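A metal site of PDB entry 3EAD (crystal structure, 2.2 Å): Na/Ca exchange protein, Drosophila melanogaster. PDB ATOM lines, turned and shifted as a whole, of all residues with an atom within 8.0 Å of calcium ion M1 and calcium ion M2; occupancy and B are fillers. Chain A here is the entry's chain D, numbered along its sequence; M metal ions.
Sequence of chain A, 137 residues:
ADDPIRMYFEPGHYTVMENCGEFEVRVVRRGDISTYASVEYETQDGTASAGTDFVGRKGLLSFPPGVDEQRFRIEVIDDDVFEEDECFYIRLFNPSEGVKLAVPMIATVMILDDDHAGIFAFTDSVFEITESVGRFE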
ATOM      1  N   MET A  17     -31.263 -22.106  28.996  1.00  0.00           N
ATOM      2  CA  MET A  17     -30.113 -22.792  29.567  1.00  0.00           C
ATOM      3  C   MET A  17     -30.496 -24.167  30.080  1.00  0.00           C
ATOM      4  O   MET A  17     -31.602 -24.353  30.594  1.00  0.00           O
ATOM      5  CB  MET A  17     -29.490 -21.942  30.664  1.00  0.00           C
ATOM      6  CG  MET A  17     -28.452 -20.999  30.138  1.00  0.00           C
ATOM      7  SD  MET A  17     -27.200 -21.920  29.212  1.00  0.00           S
ATOM      8  CE  MET A  17     -25.859 -22.031  30.397  1.00  0.00           C
ATOM      9  N   GLU A  18     -29.584 -25.132  29.942  1.00  0.00           N
ATOM     10  CA  GLU A  18     -29.848 -26.538  30.290  1.00  0.00           C
ATOM     11  C   GLU A  18     -30.008 -26.763  31.810  1.00  0.00           C
ATOM     12  O   GLU A  18     -30.536 -27.782  32.250  1.00  0.00           O
ATOM     13  CB  GLU A  18     -28.733 -27.435  29.745  1.00  0.00           C
ATOM     14  CG  GLU A  18     -29.071 -28.916  29.727  1.00  0.00           C
ATOM     15  CD  GLU A  18     -27.839 -29.790  29.782  1.00  0.00           C
ATOM     16  OE1 GLU A  18     -27.962 -31.032  29.634  1.00  0.00           O
ATOM     17  OE2 GLU A  18     -26.733 -29.244  29.990  1.00  0.00           O
ATOM     18  N   ASN A  19     -29.516 -25.789  32.572  1.00  0.00           N
ATOM     19  CA  ASN A  19     -29.704 -25.727  34.020  1.00  0.00           C
ATOM     20  C   ASN A  19     -30.535 -24.492  34.387  1.00  0.00           C
ATOM     21  O   ASN A  19     -30.048 -23.574  35.054  1.00  0.00           O
ATOM     22  CB  ASN A  19     -28.337 -25.680  34.714  1.00  0.00           C
ATOM     23  CG  ASN A  19     -27.569 -24.396  34.410  1.00  0.00           C
ATOM     24  OD1 ASN A  19     -27.390 -24.014  33.248  1.00  0.00           O
ATOM     25  ND2 ASN A  19     -27.125 -23.711  35.471  1.00  0.00           N
ATOM     26  N   THR A  52     -35.187 -37.208  28.238  1.00  0.00           N
ATOM     27  CA  THR A  52     -33.734 -36.981  28.371  1.00  0.00           C
ATOM     28  C   THR A  52     -33.290 -35.511  28.302  1.00  0.00           C
ATOM     29  O   THR A  52     -32.222 -35.165  28.825  1.00  0.00           O
ATOM     30  CB  THR A  52     -32.882 -37.867  27.400  1.00  0.00           C
ATOM     31  OG1 THR A  52     -33.059 -37.435  26.048  1.00  0.00           O
ATOM     32  CG2 THR A  52     -33.252 -39.353  27.526  1.00  0.00           C
ATOM     33  N   ASP A  53     -34.082 -34.637  27.676  1.00  0.00           N
ATOM     34  CA  ASP A  53     -33.750 -33.209  27.623  1.00  0.00           C
ATOM     35  C   ASP A  53     -34.759 -32.295  28.314  1.00  0.00           C
ATOM     36  O   ASP A  53     -34.411 -31.220  28.794  1.00  0.00           O
ATOM     37  CB  ASP A  53     -33.557 -32.758  26.177  1.00  0.00           C
ATOM     38  CG  ASP A  53     -32.324 -33.375  25.550  1.00  0.00           C
ATOM     39  OD1 ASP A  53     -32.457 -34.304  24.718  1.00  0.00           O
ATOM     40  OD2 ASP A  53     -31.213 -32.951  25.927  1.00  0.00           O
ATOM     41  N   VAL A  76     -36.835 -28.680  32.277  1.00  0.00           N
ATOM     42  CA  VAL A  76     -35.663 -29.046  31.465  1.00  0.00           C
ATOM     43  C   VAL A  76     -34.798 -30.048  32.211  1.00  0.00           C
ATOM     44  O   VAL A  76     -34.355 -29.757  33.330  1.00  0.00           O
ATOM     45  CB  VAL A  76     -34.805 -27.821  31.065  1.00  0.00           C
ATOM     46  CG1 VAL A  76     -33.458 -28.261  30.500  1.00  0.00           C
ATOM     47  CG2 VAL A  76     -35.548 -26.980  30.054  1.00  0.00           C
ATOM     48  N   ILE A  77     -34.565 -31.207  31.606  1.00  0.00           N
ATOM     49  CA  ILE A  77     -33.823 -32.278  32.284  1.00  0.00           C
ATOM     50  C   ILE A  77     -32.318 -32.049  32.242  1.00  0.00           C
ATOM     51  O   ILE A  77     -31.687 -32.104  31.183  1.00  0.00           O
ATOM     52  CB  ILE A  77     -34.226 -33.699  31.797  1.00  0.00           C
ATOM     53  CG1 ILE A  77     -35.727 -33.916  32.053  1.00  0.00           C
ATOM     54  CG2 ILE A  77     -33.377 -34.775  32.480  1.00  0.00           C
ATOM     55  CD1 ILE A  77     -36.225 -35.334  31.858  1.00  0.00           C
ATOM     56  N   ASP A  78     -31.749 -31.769  33.413  1.00  0.00           N
ATOM     57  CA  ASP A  78     -30.327 -31.506  33.546  1.00  0.00           C
ATOM     58  C   ASP A  78     -29.563 -32.819  33.667  1.00  0.00           C
ATOM     59  O   ASP A  78     -30.057 -33.791  34.255  1.00  0.00           O
ATOM     60  CB  ASP A  78     -30.070 -30.623  34.774  1.00  0.00           C
ATOM     61  CG  ASP A  78     -28.716 -29.917  34.746  1.00  0.00           C
ATOM     62  OD1 ASP A  78     -28.546 -28.957  35.564  1.00  0.00           O
ATOM     63  OD2 ASP A  78     -27.801 -30.283  33.905  1.00  0.00           O
ATOM     64  N   ASP A  79     -28.365 -32.851  33.103  1.00  0.00           N
ATOM     65  CA  ASP A  79     -27.477 -33.983  33.229  1.00  0.00           C
ATOM     66  C   ASP A  79     -26.035 -33.519  33.055  1.00  0.00           C
ATOM     67  O   ASP A  79     -25.781 -32.323  32.751  1.00  0.00           O
ATOM     68  CB  ASP A  79     -27.837 -35.095  32.228  1.00  0.00           C
ATOM     69  CG  ASP A  79     -27.596 -34.700  30.770  1.00  0.00           C
ATOM     70  OD1 ASP A  79     -27.790 -35.563  29.882  1.00  0.00           O
ATOM     71  OD2 ASP A  79     -27.196 -33.541  30.490  1.00  0.00           O
ATOM     72  N   ASP A  80     -25.089 -34.464  33.234  1.00  0.00           N
ATOM     73  CA  ASP A  80     -23.671 -34.136  33.178  1.00  0.00           C
ATOM     74  C   ASP A  80     -22.987 -34.700  31.930  1.00  0.00           C
ATOM     75  O   ASP A  80     -22.013 -35.458  32.028  1.00  0.00           O
ATOM     76  CB  ASP A  80     -22.988 -34.605  34.458  1.00  0.00           C
ATOM     77  CG  ASP A  80     -22.184 -33.501  35.129  1.00  0.00           C
ATOM     78  OD1 ASP A  80     -20.793 -33.628  35.065  1.00  0.00           O
ATOM     79  OD2 ASP A  80     -22.904 -32.516  35.729  1.00  0.00           O
ATOM     80  N   VAL A  81     -23.506 -34.336  30.757  1.00  0.00           N
ATOM     81  CA  VAL A  81     -22.934 -34.732  29.449  1.00  0.00           C
ATOM     82  C   VAL A  81     -23.012 -33.579  28.426  1.00  0.00           C
ATOM     83  O   VAL A  81     -24.059 -32.948  28.256  1.00  0.00           O
ATOM     84  CB  VAL A  81     -23.578 -36.055  28.881  1.00  0.00           C
ATOM     85  CG1 VAL A  81     -23.040 -36.377  27.477  1.00  0.00           C
ATOM     86  CG2 VAL A  81     -23.330 -37.249  29.819  1.00  0.00           C
ATOM     87  N   PHE A  82     -21.886 -33.299  27.758  1.00  0.00           N
ATOM     88  CA  PHE A  82     -21.760 -32.202  26.798  1.00  0.00           C
ATOM     89  C   PHE A  82     -22.465 -32.499  25.493  1.00  0.00           C
ATOM     90  O   PHE A  82     -22.327 -33.579  24.914  1.00  0.00           O
ATOM     91  CB  PHE A  82     -20.282 -31.861  26.559  1.00  0.00           C
ATOM     92  CG  PHE A  82     -19.949 -31.429  25.146  1.00  0.00           C
ATOM     93  CD1 PHE A  82     -19.139 -32.231  24.341  1.00  0.00           C
ATOM     94  CD2 PHE A  82     -20.415 -30.220  24.626  1.00  0.00           C
ATOM     95  CE1 PHE A  82     -18.823 -31.846  23.030  1.00  0.00           C
ATOM     96  CE2 PHE A  82     -20.116 -29.825  23.325  1.00  0.00           C
ATOM     97  CZ  PHE A  82     -19.314 -30.640  22.530  1.00  0.00           C
ATOM     98  N   GLU A  83     -23.221 -31.501  25.040  1.00  0.00           N
ATOM     99  CA  GLU A  83     -24.020 -31.576  23.810  1.00  0.00           C
ATOM    100  C   GLU A  83     -23.871 -30.303  22.957  1.00  0.00           C
ATOM    101  O   GLU A  83     -23.384 -29.260  23.442  1.00  0.00           O
ATOM    102  CB  GLU A  83     -25.512 -31.775  24.146  1.00  0.00           C
ATOM    103  CG  GLU A  83     -25.791 -32.676  25.338  1.00  0.00           C
ATOM    104  CD  GLU A  83     -27.211 -32.534  25.841  1.00  0.00           C
ATOM    105  OE1 GLU A  83     -27.663 -31.398  26.116  1.00  0.00           O
ATOM    106  OE2 GLU A  83     -27.891 -33.577  25.959  1.00  0.00           O
ATOM    107  N   GLU A  84     -24.287 -30.390  21.695  1.00  0.00           N
ATOM    108  CA  GLU A  84     -24.482 -29.204  20.870  1.00  0.00           C
ATOM    109  C   GLU A  84     -25.873 -28.651  21.133  1.00  0.00           C
ATOM    110  O   GLU A  84     -26.688 -29.324  21.780  1.00  0.00           O
ATOM    111  CB  GLU A  84     -24.287 -29.527  19.377  1.00  0.00           C
ATOM    112  CG  GLU A  84     -22.827 -29.728  18.985  1.00  0.00           C
ATOM    113  CD  GLU A  84     -22.570 -29.526  17.500  1.00  0.00           C
ATOM    114  OE1 GLU A  84     -23.536 -29.362  16.722  1.00  0.00           O
ATOM    115  OE2 GLU A  84     -21.382 -29.522  17.107  1.00  0.00           O
ATOM    116  N   GLU A  86     -29.577 -27.919  21.095  1.00  0.00           N
ATOM    117  CA  GLU A  86     -30.686 -28.771  20.674  1.00  0.00           C
ATOM    118  C   GLU A  86     -32.005 -28.012  20.623  1.00  0.00           C
ATOM    119  O   GLU A  86     -32.126 -26.941  21.192  1.00  0.00           O
ATOM    120  CB  GLU A  86     -30.798 -30.018  21.567  1.00  0.00           C
ATOM    121  CG  GLU A  86     -29.631 -30.976  21.394  1.00  0.00           C
ATOM    122  CD  GLU A  86     -29.741 -32.227  22.263  1.00  0.00           C
ATOM    123  OE1 GLU A  86     -30.679 -32.302  23.077  1.00  0.00           O
ATOM    124  OE2 GLU A  86     -28.885 -33.128  22.110  1.00  0.00           O
ATOM    125  N   ILE A 111     -32.419 -25.318  23.646  1.00  0.00           N
ATOM    126  CA  ILE A 111     -31.617 -25.617  24.828  1.00  0.00           C
ATOM    127  C   ILE A 111     -30.111 -25.416  24.587  1.00  0.00           C
ATOM    128  O   ILE A 111     -29.487 -26.082  23.761  1.00  0.00           O
ATOM    129  CB  ILE A 111     -31.872 -27.051  25.376  1.00  0.00           C
ATOM    130  CG1 ILE A 111     -33.381 -27.401  25.334  1.00  0.00           C
ATOM    131  CG2 ILE A 111     -31.284 -27.204  26.807  1.00  0.00           C
ATOM    132  CD1 ILE A 111     -33.742 -28.878  25.571  1.00  0.00           C
ATOM    133  N   LEU A 112     -29.534 -24.467  25.322  1.00  0.00           N
ATOM    134  CA  LEU A 112     -28.093 -24.259  25.307  1.00  0.00           C
ATOM    135  C   LEU A 112     -27.455 -25.205  26.332  1.00  0.00           C
ATOM    136  O   LEU A 112     -27.827 -25.199  27.515  1.00  0.00           O
ATOM    137  CB  LEU A 112     -27.758 -22.792  25.667  1.00  0.00           C
ATOM    138  CG  LEU A 112     -28.249 -21.650  24.766  1.00  0.00           C
ATOM    139  CD1 LEU A 112     -28.149 -20.314  25.478  1.00  0.00           C
ATOM    140  CD2 LEU A 112     -27.475 -21.609  23.453  1.00  0.00           C
ATOM    141  N   ASP A 113     -26.512 -26.036  25.859  1.00  0.00           N
ATOM    142  CA  ASP A 113     -25.741 -26.918  26.746  1.00  0.00           C
ATOM    143  C   ASP A 113     -24.675 -26.130  27.518  1.00  0.00           C
ATOM    144  O   ASP A 113     -24.041 -25.220  26.970  1.00  0.00           O
ATOM    145  CB  ASP A 113     -25.103 -28.075  25.940  1.00  0.00           C
ATOM    146  CG  ASP A 113     -24.387 -29.098  26.833  1.00  0.00           C
ATOM    147  OD1 ASP A 113     -25.052 -29.802  27.628  1.00  0.00           O
ATOM    148  OD2 ASP A 113     -23.152 -29.225  26.691  1.00  0.00           O
ATOM    149  N   ASP A 114     -24.512 -26.465  28.795  1.00  0.00           N
ATOM    150  CA  ASP A 114     -23.578 -25.753  29.678  1.00  0.00           C
ATOM    151  C   ASP A 114     -22.221 -26.454  29.913  1.00  0.00           C
ATOM    152  O   ASP A 114     -21.230 -25.808  30.263  1.00  0.00           O
ATOM    153  CB  ASP A 114     -24.264 -25.373  31.022  1.00  0.00           C
ATOM    154  CG  ASP A 114     -24.508 -26.595  31.960  1.00  0.00           C
ATOM    155  OD1 ASP A 114     -24.072 -27.841  31.564  1.00  0.00           O
ATOM    156  OD2 ASP A 114     -25.256 -26.274  33.027  1.00  0.00           O
ATOM    157  N   ASP A 115     -22.200 -27.770  29.699  1.00  0.00           N
ATOM    158  CA  ASP A 115     -21.025 -28.598  29.913  1.00  0.00           C
ATOM    159  C   ASP A 115     -19.986 -28.425  28.817  1.00  0.00           C
ATOM    160  O   ASP A 115     -19.683 -27.306  28.392  1.00  0.00           O
ATOM    161  CB  ASP A 115     -21.453 -30.065  29.999  1.00  0.00           C
ATOM    162  CG  ASP A 115     -22.411 -30.327  31.148  1.00  0.00           C
ATOM    163  OD1 ASP A 115     -21.947 -30.259  32.341  1.00  0.00           O
ATOM    164  OD2 ASP A 115     -23.615 -30.595  30.856  1.00  0.00           O
HETATM  165 CA    CA M   1     -26.123 -32.199  29.105  1.00  0.00          CA
HETATM  166 CA    CA M   2     -25.967 -29.826  32.395  1.00  0.00          CA
HETATM  167 CA    CA M   3     -29.796 -31.815  27.446  1.00  0.00          CA
HETATM  168 CA    CA M   4     -29.893 -34.771  23.929  1.00  0.00          CA
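The side-chain carboxylate (OD2) of Asp 79 is bound to calcium ion M1 (2.2 Å).
The side-chain carboxylate (OE1) of Glu 18 binds calcium ion M1 (2.2 Å).
Calcium ion M1 is bound by the backbone carbonyl oxygen (O) of Val 81.
Slightly farther from calcium ion M1 lies the side-chain carboxylate (OD1) of Asp 113 (3.0 Å).
Slightly farther from calcium ion M1 lies OE2 of Glu 18 (3.1 Å).
N of Glu 18 sits at hydrogen-bond distance from O of Leu 112 (3.0 Å).
OD2 of Asp 113 lies within hydrogen-bond range of N of Glu 83.
OD2 of Asp 113 sits at hydrogen-bond distance from N of Asp 115 (3.5 Å).
OD2 of Asp 114 lies close to OD1 of Asn 19 (3.1 Å).
Residues that only touch calcium ion M1: Glu 83.
Six residues have an atom within 4 Å of calcium ion M1: Glu 18, Asp 79, Val 81, Glu 83, Asp 113 and Asp 115.
The nearest printed residue that does not touch calcium ion M1 is Phe 82 (4.6 Å).
OD2 of Asp 78 binds calcium ion M2 (2.4 Å).
The backbone carbonyl oxygen (O) of Asp 79 binds calcium ion M2 (2.5 Å).
Calcium ion M2 is bound by the side-chain carboxylate (OE2) of Glu 18 (2.6 Å).
Calcium ion M2 is bound by OD1 of Asp 114 (2.9 Å).
Slightly farther from calcium ion M2 lies OD2 of Asp 115 (2.9 Å).
Five residues have an atom within 4 Å of calcium ion M2: Glu 18, Asp 78, Asp 79, Asp 114 and Asp 115.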
